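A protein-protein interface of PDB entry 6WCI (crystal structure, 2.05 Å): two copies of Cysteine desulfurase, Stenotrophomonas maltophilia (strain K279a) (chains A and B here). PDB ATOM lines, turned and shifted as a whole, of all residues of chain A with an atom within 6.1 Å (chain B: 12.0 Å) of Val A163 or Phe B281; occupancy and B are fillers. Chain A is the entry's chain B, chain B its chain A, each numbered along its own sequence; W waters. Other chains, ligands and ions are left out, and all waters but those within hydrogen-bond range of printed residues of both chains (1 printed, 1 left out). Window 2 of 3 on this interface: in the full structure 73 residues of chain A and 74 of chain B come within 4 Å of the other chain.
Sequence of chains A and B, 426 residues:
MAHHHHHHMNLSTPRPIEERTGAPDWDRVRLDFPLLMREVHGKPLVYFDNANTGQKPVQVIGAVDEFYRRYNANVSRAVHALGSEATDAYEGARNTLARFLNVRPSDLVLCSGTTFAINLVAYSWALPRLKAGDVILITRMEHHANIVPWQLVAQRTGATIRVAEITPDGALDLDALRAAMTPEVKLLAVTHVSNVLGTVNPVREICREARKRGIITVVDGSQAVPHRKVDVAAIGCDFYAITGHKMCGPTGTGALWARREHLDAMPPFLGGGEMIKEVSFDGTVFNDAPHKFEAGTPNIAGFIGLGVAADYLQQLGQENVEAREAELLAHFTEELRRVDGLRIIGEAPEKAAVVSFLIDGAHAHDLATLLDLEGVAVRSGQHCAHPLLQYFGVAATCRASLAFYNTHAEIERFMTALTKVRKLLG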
ATOM      1  N   ILE A 136      -5.674   9.198  -6.694  1.00  0.00           N
ATOM      2  CA  ILE A 136      -5.022   8.459  -7.764  1.00  0.00           C
ATOM      3  C   ILE A 136      -5.497   7.015  -7.660  1.00  0.00           C
ATOM      4  O   ILE A 136      -5.360   6.378  -6.607  1.00  0.00           O
ATOM      5  CB  ILE A 136      -3.492   8.536  -7.659  1.00  0.00           C
ATOM      6  CG1 ILE A 136      -3.010   9.994  -7.659  1.00  0.00           C
ATOM      7  CG2 ILE A 136      -2.824   7.726  -8.782  1.00  0.00           C
ATOM      8  CD1 ILE A 136      -1.536  10.139  -7.341  1.00  0.00           C
ATOM      9  N   LEU A 137      -6.065   6.500  -8.737  1.00  0.00           N
ATOM     10  CA  LEU A 137      -6.621   5.151  -8.742  1.00  0.00           C
ATOM     11  C   LEU A 137      -5.633   4.246  -9.468  1.00  0.00           C
ATOM     12  O   LEU A 137      -5.248   4.535 -10.606  1.00  0.00           O
ATOM     13  CB  LEU A 137      -7.997   5.136  -9.407  1.00  0.00           C
ATOM     14  CG  LEU A 137      -8.788   3.826  -9.344  1.00  0.00           C
ATOM     15  CD1 LEU A 137      -9.083   3.460  -7.902  1.00  0.00           C
ATOM     16  CD2 LEU A 137     -10.078   3.928 -10.143  1.00  0.00           C
ATOM     17  N   ILE A 138      -5.191   3.184  -8.791  1.00  0.00           N
ATOM     18  CA  ILE A 138      -4.161   2.270  -9.286  1.00  0.00           C
ATOM     19  C   ILE A 138      -4.701   0.855  -9.172  1.00  0.00           C
ATOM     20  O   ILE A 138      -5.233   0.489  -8.120  1.00  0.00           O
ATOM     21  CB  ILE A 138      -2.856   2.387  -8.473  1.00  0.00           C
ATOM     22  CG1 ILE A 138      -2.436   3.860  -8.316  1.00  0.00           C
ATOM     23  CG2 ILE A 138      -1.755   1.505  -9.077  1.00  0.00           C
ATOM     24  CD1 ILE A 138      -1.216   4.046  -7.436  1.00  0.00           C
ATOM     25  N   THR A 139      -4.543   0.047 -10.223  1.00  0.00           N
ATOM     26  CA  THR A 139      -5.103  -1.305 -10.160  1.00  0.00           C
ATOM     27  C   THR A 139      -4.232  -2.222  -9.310  1.00  0.00           C
ATOM     28  O   THR A 139      -3.018  -2.033  -9.186  1.00  0.00           O
ATOM     29  CB  THR A 139      -5.268  -1.936 -11.545  1.00  0.00           C
ATOM     30  OG1 THR A 139      -4.108  -2.718 -11.859  1.00  0.00           O
ATOM     31  CG2 THR A 139      -5.478  -0.889 -12.609  1.00  0.00           C
ATOM     32  N   ARG A 140      -4.882  -3.234  -8.731  1.00  0.00           N
ATOM     33  CA  ARG A 140      -4.221  -4.242  -7.909  1.00  0.00           C
ATOM     34  C   ARG A 140      -3.092  -4.970  -8.638  1.00  0.00           C
ATOM     35  O   ARG A 140      -2.180  -5.487  -7.982  1.00  0.00           O
ATOM     36  CB  ARG A 140      -5.283  -5.246  -7.432  1.00  0.00           C
ATOM     37  CG  ARG A 140      -4.769  -6.460  -6.693  1.00  0.00           C
ATOM     38  CD  ARG A 140      -4.071  -6.071  -5.408  1.00  0.00           C
ATOM     39  NE  ARG A 140      -4.964  -5.377  -4.487  1.00  0.00           N
ATOM     40  CZ  ARG A 140      -4.635  -5.067  -3.240  1.00  0.00           C
ATOM     41  NH1 ARG A 140      -3.437  -5.401  -2.771  1.00  0.00           N
ATOM     42  NH2 ARG A 140      -5.496  -4.421  -2.467  1.00  0.00           N
ATOM     43  N   GLU A 142      -0.925  -3.746 -10.999  1.00  0.00           N
ATOM     44  CA  GLU A 142       0.117  -2.898 -11.568  1.00  0.00           C
ATOM     45  C   GLU A 142       1.503  -3.358 -11.141  1.00  0.00           C
ATOM     46  O   GLU A 142       1.700  -3.911 -10.057  1.00  0.00           O
ATOM     47  CB  GLU A 142      -0.068  -1.435 -11.146  1.00  0.00           C
ATOM     48  CG  GLU A 142      -1.315  -0.797 -11.731  1.00  0.00           C
ATOM     49  CD  GLU A 142      -1.428  -1.060 -13.224  1.00  0.00           C
ATOM     50  OE1 GLU A 142      -0.533  -0.613 -13.983  1.00  0.00           O
ATOM     51  OE2 GLU A 142      -2.400  -1.732 -13.631  1.00  0.00           O
ATOM     52  N   ILE A 147       3.254   2.091  -9.723  1.00  0.00           N
ATOM     53  CA  ILE A 147       2.768   2.291  -8.362  1.00  0.00           C
ATOM     54  C   ILE A 147       3.642   3.320  -7.660  1.00  0.00           C
ATOM     55  O   ILE A 147       3.153   4.350  -7.195  1.00  0.00           O
ATOM     56  CB  ILE A 147       2.760   0.980  -7.562  1.00  0.00           C
ATOM     57  CG1 ILE A 147       1.795  -0.030  -8.188  1.00  0.00           C
ATOM     58  CG2 ILE A 147       2.447   1.264  -6.096  1.00  0.00           C
ATOM     59  CD1 ILE A 147       1.863  -1.436  -7.578  1.00  0.00           C
ATOM     60  N   GLN A 151       3.085   6.924  -5.495  1.00  0.00           N
ATOM     61  CA  GLN A 151       3.309   7.045  -4.060  1.00  0.00           C
ATOM     62  C   GLN A 151       4.219   8.221  -3.728  1.00  0.00           C
ATOM     63  O   GLN A 151       4.059   8.858  -2.680  1.00  0.00           O
ATOM     64  CB  GLN A 151       3.895   5.745  -3.519  1.00  0.00           C
ATOM     65  CG  GLN A 151       2.864   4.617  -3.479  1.00  0.00           C
ATOM     66  CD  GLN A 151       3.446   3.320  -2.988  1.00  0.00           C
ATOM     67  OE1 GLN A 151       4.553   2.942  -3.374  1.00  0.00           O
ATOM     68  NE2 GLN A 151       2.703   2.621  -2.134  1.00  0.00           N
ATOM     69  N   ILE A 161      -4.178   7.476  -2.566  1.00  0.00           N
ATOM     70  CA  ILE A 161      -4.181   6.384  -3.530  1.00  0.00           C
ATOM     71  C   ILE A 161      -5.306   5.424  -3.176  1.00  0.00           C
ATOM     72  O   ILE A 161      -5.445   5.019  -2.015  1.00  0.00           O
ATOM     73  CB  ILE A 161      -2.824   5.666  -3.547  1.00  0.00           C
ATOM     74  CG1 ILE A 161      -1.752   6.578  -4.165  1.00  0.00           C
ATOM     75  CG2 ILE A 161      -2.928   4.346  -4.297  1.00  0.00           C
ATOM     76  CD1 ILE A 161      -0.427   5.903  -4.329  1.00  0.00           C
ATOM     77  N   ARG A 162      -6.105   5.056  -4.175  1.00  0.00           N
ATOM     78  CA  ARG A 162      -7.186   4.092  -4.020  1.00  0.00           C
ATOM     79  C   ARG A 162      -6.952   2.950  -4.998  1.00  0.00           C
ATOM     80  O   ARG A 162      -6.435   3.163  -6.096  1.00  0.00           O
ATOM     81  CB  ARG A 162      -8.544   4.770  -4.267  1.00  0.00           C
ATOM     82  CG  ARG A 162      -9.759   3.872  -4.187  1.00  0.00           C
ATOM     83  CD  ARG A 162     -10.996   4.646  -4.602  1.00  0.00           C
ATOM     84  NE  ARG A 162     -11.245   5.790  -3.728  1.00  0.00           N
ATOM     85  CZ  ARG A 162     -12.095   6.772  -4.016  1.00  0.00           C
ATOM     86  NH1 ARG A 162     -12.761   6.739  -5.164  1.00  0.00           N
ATOM     87  NH2 ARG A 162     -12.276   7.786  -3.166  1.00  0.00           N
ATOM     88  N   VAL A 163      -7.311   1.728  -4.600  1.00  0.00           N
ATOM     89  CA  VAL A 163      -6.955   0.527  -5.363  1.00  0.00           C
ATOM     90  C   VAL A 163      -8.157   0.042  -6.160  1.00  0.00           C
ATOM     91  O   VAL A 163      -9.267  -0.059  -5.628  1.00  0.00           O
ATOM     92  CB  VAL A 163      -6.430  -0.595  -4.448  1.00  0.00           C
ATOM     93  CG1 VAL A 163      -6.042  -1.825  -5.290  1.00  0.00           C
ATOM     94  CG2 VAL A 163      -5.233  -0.123  -3.652  1.00  0.00           C
ATOM     95  N   ALA A 164      -7.935  -0.267  -7.436  1.00  0.00           N
ATOM     96  CA  ALA A 164      -8.941  -0.915  -8.269  1.00  0.00           C
ATOM     97  C   ALA A 164      -8.731  -2.429  -8.223  1.00  0.00           C
ATOM     98  O   ALA A 164      -7.676  -2.924  -8.632  1.00  0.00           O
ATOM     99  CB  ALA A 164      -8.864  -0.385  -9.702  1.00  0.00           C
ATOM    100  N   GLU A 165      -9.734  -3.165  -7.734  1.00  0.00           N
ATOM    101  CA  GLU A 165      -9.518  -4.563  -7.392  1.00  0.00           C
ATOM    102  C   GLU A 165      -9.635  -5.473  -8.612  1.00  0.00           C
ATOM    103  O   GLU A 165     -10.124  -5.093  -9.678  1.00  0.00           O
ATOM    104  CB  GLU A 165     -10.512  -5.030  -6.315  1.00  0.00           C
ATOM    105  CG  GLU A 165     -10.233  -4.533  -4.891  1.00  0.00           C
ATOM    106  CD  GLU A 165      -8.751  -4.614  -4.482  1.00  0.00           C
ATOM    107  OE1 GLU A 165      -7.999  -5.471  -5.004  1.00  0.00           O
ATOM    108  OE2 GLU A 165      -8.337  -3.802  -3.621  1.00  0.00           O
ATOM    109  N   ALA A 180     -15.463   2.839  -8.417  1.00  0.00           N
ATOM    110  CA  ALA A 180     -14.306   3.506  -7.834  1.00  0.00           C
ATOM    111  C   ALA A 180     -13.972   4.827  -8.512  1.00  0.00           C
ATOM    112  O   ALA A 180     -13.232   5.630  -7.931  1.00  0.00           O
ATOM    113  CB  ALA A 180     -13.078   2.593  -7.899  1.00  0.00           C
ATOM    114  N   PRO A 387       1.892  -5.949  -4.322  1.00  0.00           N
ATOM    115  CA  PRO A 387       0.490  -5.905  -3.870  1.00  0.00           C
ATOM    116  C   PRO A 387      -0.384  -6.934  -4.551  1.00  0.00           C
ATOM    117  O   PRO A 387      -1.325  -7.434  -3.926  1.00  0.00           O
ATOM    118  CB  PRO A 387       0.047  -4.474  -4.211  1.00  0.00           C
ATOM    119  CG  PRO A 387       1.311  -3.708  -4.405  1.00  0.00           C
ATOM    120  CD  PRO A 387       2.276  -4.693  -4.986  1.00  0.00           C
ATOM    121  N   LEU A 388      -0.099  -7.274  -5.812  1.00  0.00           N
ATOM    122  CA  LEU A 388      -0.850  -8.326  -6.485  1.00  0.00           C
ATOM    123  C   LEU A 388      -0.701  -9.652  -5.750  1.00  0.00           C
ATOM    124  O   LEU A 388      -1.694 -10.338  -5.477  1.00  0.00           O
ATOM    125  CB  LEU A 388      -0.395  -8.450  -7.938  1.00  0.00           C
ATOM    126  CG  LEU A 388      -1.015  -9.606  -8.733  1.00  0.00           C
ATOM    127  CD1 LEU A 388      -2.535  -9.481  -8.788  1.00  0.00           C
ATOM    128  CD2 LEU A 388      -0.419  -9.672 -10.129  1.00  0.00           C
ATOM    129  N   ILE B 276      13.091  -0.192  -4.659  1.00  0.00           N
ATOM    130  CA  ILE B 276      12.272  -0.508  -3.501  1.00  0.00           C
ATOM    131  C   ILE B 276      12.823  -1.753  -2.825  1.00  0.00           C
ATOM    132  O   ILE B 276      13.505  -2.587  -3.431  1.00  0.00           O
ATOM    133  CB  ILE B 276      10.782  -0.721  -3.862  1.00  0.00           C
ATOM    134  CG1 ILE B 276      10.655  -1.799  -4.951  1.00  0.00           C
ATOM    135  CG2 ILE B 276      10.129   0.586  -4.281  1.00  0.00           C
ATOM    136  CD1 ILE B 276      10.334  -3.200  -4.406  1.00  0.00           C
ATOM    137  N   LYS B 277      12.494  -1.888  -1.550  1.00  0.00           N
ATOM    138  CA  LYS B 277      12.663  -3.122  -0.803  1.00  0.00           C
ATOM    139  C   LYS B 277      11.339  -3.835  -0.584  1.00  0.00           C
ATOM    140  O   LYS B 277      11.227  -5.036  -0.857  1.00  0.00           O
ATOM    141  CB  LYS B 277      13.326  -2.810   0.539  1.00  0.00           C
ATOM    142  CG  LYS B 277      13.618  -4.000   1.412  1.00  0.00           C
ATOM    143  CD  LYS B 277      14.275  -3.514   2.688  1.00  0.00           C
ATOM    144  CE  LYS B 277      15.418  -2.551   2.358  1.00  0.00           C
ATOM    145  NZ  LYS B 277      15.835  -1.715   3.521  1.00  0.00           N
ATOM    146  N   GLU B 278      10.323  -3.112  -0.105  1.00  0.00           N
ATOM    147  CA  GLU B 278       8.986  -3.666   0.090  1.00  0.00           C
ATOM    148  C   GLU B 278       7.975  -2.651  -0.416  1.00  0.00           C
ATOM    149  O   GLU B 278       8.058  -1.473  -0.066  1.00  0.00           O
ATOM    150  CB  GLU B 278       8.701  -3.977   1.570  1.00  0.00           C
ATOM    151  CG  GLU B 278       9.777  -4.783   2.294  1.00  0.00           C
ATOM    152  CD  GLU B 278       9.931  -6.204   1.763  1.00  0.00           C
ATOM    153  OE1 GLU B 278       9.082  -6.654   0.962  1.00  0.00           O
ATOM    154  OE2 GLU B 278      10.912  -6.877   2.153  1.00  0.00           O
ATOM    155  N   VAL B 279       7.028  -3.095  -1.236  1.00  0.00           N
ATOM    156  CA  VAL B 279       5.980  -2.228  -1.764  1.00  0.00           C
ATOM    157  C   VAL B 279       4.641  -2.683  -1.207  1.00  0.00           C
ATOM    158  O   VAL B 279       4.304  -3.872  -1.267  1.00  0.00           O
ATOM    159  CB  VAL B 279       5.966  -2.226  -3.305  1.00  0.00           C
ATOM    160  CG1 VAL B 279       4.713  -1.514  -3.823  1.00  0.00           C
ATOM    161  CG2 VAL B 279       7.212  -1.548  -3.845  1.00  0.00           C
ATOM    162  N   SER B 280       3.885  -1.737  -0.657  1.00  0.00           N
ATOM    163  CA  SER B 280       2.513  -1.985  -0.263  1.00  0.00           C
ATOM    164  C   SER B 280       1.715  -0.708  -0.457  1.00  0.00           C
ATOM    165  O   SER B 280       2.248   0.397  -0.333  1.00  0.00           O
ATOM    166  CB  SER B 280       2.410  -2.438   1.194  1.00  0.00           C
ATOM    167  OG  SER B 280       1.069  -2.385   1.621  1.00  0.00           O
ATOM    168  N   PHE B 281       0.427  -0.866  -0.744  1.00  0.00           N
ATOM    169  CA  PHE B 281      -0.412   0.317  -0.873  1.00  0.00           C
ATOM    170  C   PHE B 281      -0.565   1.046   0.456  1.00  0.00           C
ATOM    171  O   PHE B 281      -0.931   2.225   0.460  1.00  0.00           O
ATOM    172  CB  PHE B 281      -1.773  -0.060  -1.451  1.00  0.00           C
ATOM    173  CG  PHE B 281      -1.743  -0.329  -2.929  1.00  0.00           C
ATOM    174  CD1 PHE B 281      -1.391   0.677  -3.820  1.00  0.00           C
ATOM    175  CD2 PHE B 281      -2.076  -1.579  -3.429  1.00  0.00           C
ATOM    176  CE1 PHE B 281      -1.360   0.441  -5.187  1.00  0.00           C
ATOM    177  CE2 PHE B 281      -2.059  -1.820  -4.789  1.00  0.00           C
ATOM    178  CZ  PHE B 281      -1.699  -0.814  -5.673  1.00  0.00           C
ATOM    179  N   ASP B 282      -0.273   0.379   1.576  1.00  0.00           N
ATOM    180  CA  ASP B 282      -0.220   1.029   2.881  1.00  0.00           C
ATOM    181  C   ASP B 282       1.062   1.819   3.104  1.00  0.00           C
ATOM    182  O   ASP B 282       1.114   2.638   4.027  1.00  0.00           O
ATOM    183  CB  ASP B 282      -0.350  -0.009   3.992  1.00  0.00           C
ATOM    184  CG  ASP B 282      -1.702  -0.657   4.012  1.00  0.00           C
ATOM    185  OD1 ASP B 282      -2.686   0.053   3.723  1.00  0.00           O
ATOM    186  OD2 ASP B 282      -1.778  -1.871   4.307  1.00  0.00           O
ATOM    187  N   GLY B 283       2.094   1.577   2.297  1.00  0.00           N
ATOM    188  CA  GLY B 283       3.373   2.245   2.458  1.00  0.00           C
ATOM    189  C   GLY B 283       4.508   1.406   1.905  1.00  0.00           C
ATOM    190  O   GLY B 283       4.490   0.179   2.028  1.00  0.00           O
ATOM    191  N   THR B 284       5.496   2.050   1.287  1.00  0.00           N
ATOM    192  CA  THR B 284       6.616   1.365   0.659  1.00  0.00           C
ATOM    193  C   THR B 284       7.901   1.657   1.428  1.00  0.00           C
ATOM    194  O   THR B 284       8.084   2.756   1.960  1.00  0.00           O
ATOM    195  CB  THR B 284       6.730   1.790  -0.816  1.00  0.00           C
ATOM    196  OG1 THR B 284       5.711   1.120  -1.572  1.00  0.00           O
ATOM    197  CG2 THR B 284       8.113   1.484  -1.416  1.00  0.00           C
ATOM    198  N   VAL B 285       8.769   0.653   1.519  1.00  0.00           N
ATOM    199  CA  VAL B 285      10.076   0.777   2.149  1.00  0.00           C
ATOM    200  C   VAL B 285      11.115   0.768   1.040  1.00  0.00           C
ATOM    201  O   VAL B 285      11.075  -0.092   0.151  1.00  0.00           O
ATOM    202  CB  VAL B 285      10.322  -0.355   3.164  1.00  0.00           C
ATOM    203  CG1 VAL B 285      11.687  -0.203   3.829  1.00  0.00           C
ATOM    204  CG2 VAL B 285       9.208  -0.386   4.206  1.00  0.00           C
ATOM    205  N   PHE B 286      12.020   1.736   1.063  1.00  0.00           N
ATOM    206  CA  PHE B 286      12.957   1.896  -0.037  1.00  0.00           C
ATOM    207  C   PHE B 286      14.286   1.227   0.282  1.00  0.00           C
ATOM    208  O   PHE B 286      14.629   0.978   1.441  1.00  0.00           O
ATOM    209  CB  PHE B 286      13.162   3.379  -0.364  1.00  0.00           C
ATOM    210  CG  PHE B 286      11.905   4.063  -0.823  1.00  0.00           C
ATOM    211  CD1 PHE B 286      11.469   3.929  -2.130  1.00  0.00           C
ATOM    212  CD2 PHE B 286      11.138   4.803   0.068  1.00  0.00           C
ATOM    213  CE1 PHE B 286      10.290   4.531  -2.553  1.00  0.00           C
ATOM    214  CE2 PHE B 286       9.970   5.418  -0.352  1.00  0.00           C
ATOM    215  CZ  PHE B 286       9.537   5.272  -1.658  1.00  0.00           C
HETATM  216  O   HOH W   1       0.102   3.728  -1.306  1.00  0.00           O
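O of Ser B280 is in hydrogen-bond range of NE2 of Gln A151, at 2.9 Å.
The side-chain hydroxyl (OG1) of Thr B284 lies within hydrogen-bond range of the side-chain amide oxygen (OE1) of Gln A151 (2.8 Å).
No position is printed for both chains.
Of the 6 pairs that touch across the chains among the printed residues, none has its exchanged pair printed and touching as well.
The side-chain hydroxyl (OG) of Ser B280 lies close to the backbone NH (N) of Asp B282 (3.1 Å).
The side-chain hydroxyl (OG1) of Thr A139 lies within hydrogen-bond range of the side-chain carboxylate (OE2) of Glu A142 (2.7 Å).
The backbone carbonyl oxygen (O) of Pro A387 sits at hydrogen-bond distance from the guanidinium group (NH1) of Arg A140 (3.2 Å).
No residue of chain B comes within 4 Å of Ile A138.
No residue of chain B comes within 4 Å of Arg A140.
Of the printed residues of chain B, Ile A147 touches Phe B281.
Of the printed residues of chain B, Gln A151 touches Ser B280 and Thr B284.
Val A163 touches one residue of chain B.
Glu A165 touches none of the printed residues of chain B.
No residue of chain B comes within 4 Å of Ala A180.
Pro A387 touches just one residue of chain B: Phe B281 (3.4 Å).
Leu A388 touches none of the printed residues of chain B.
Glu B278 touches none of the printed residues of chain A.
Of the printed residues of chain A, Ser B280 touches Gln A151 (2.9 Å).
Of the printed residues of chain A, Phe B281 touches Thr A139 (3.9 Å), Ile A147 (3.9996 Å), Val A163 (3.5 Å) and Pro A387 (3.4 Å).
Of the printed residues of chain A, Thr B284 touches Gln A151 (2.8 Å).
Water W1 lies within hydrogen-bond range of O of Phe B281 (2.5 Å) and NE2 of Gln A151 (2.9 Å).
Of the 16 printed residues of chain A, 5 touch a printed residue of chain B.
Printed residues of chain A that touch a printed residue of chain B: Thr A139, Ile A147, Gln A151, Val A163 and Pro A387.
Hydrophobic or aromatic side chains of chain A that line the printed part of chain B: Ile A147, Val A163 and Pro A387.
Among the printed residues, 6 pairs touch across the chains.
Thr A139 touches Phe B281 (O to CZ, 3.9 Å).
Ile A147 touches Phe B281.
Phe B281 touches Val A163 (CD2 to CG2, 3.5 Å).
Pro A387 touches Phe B281 (CB to CE2, 3.4 Å).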
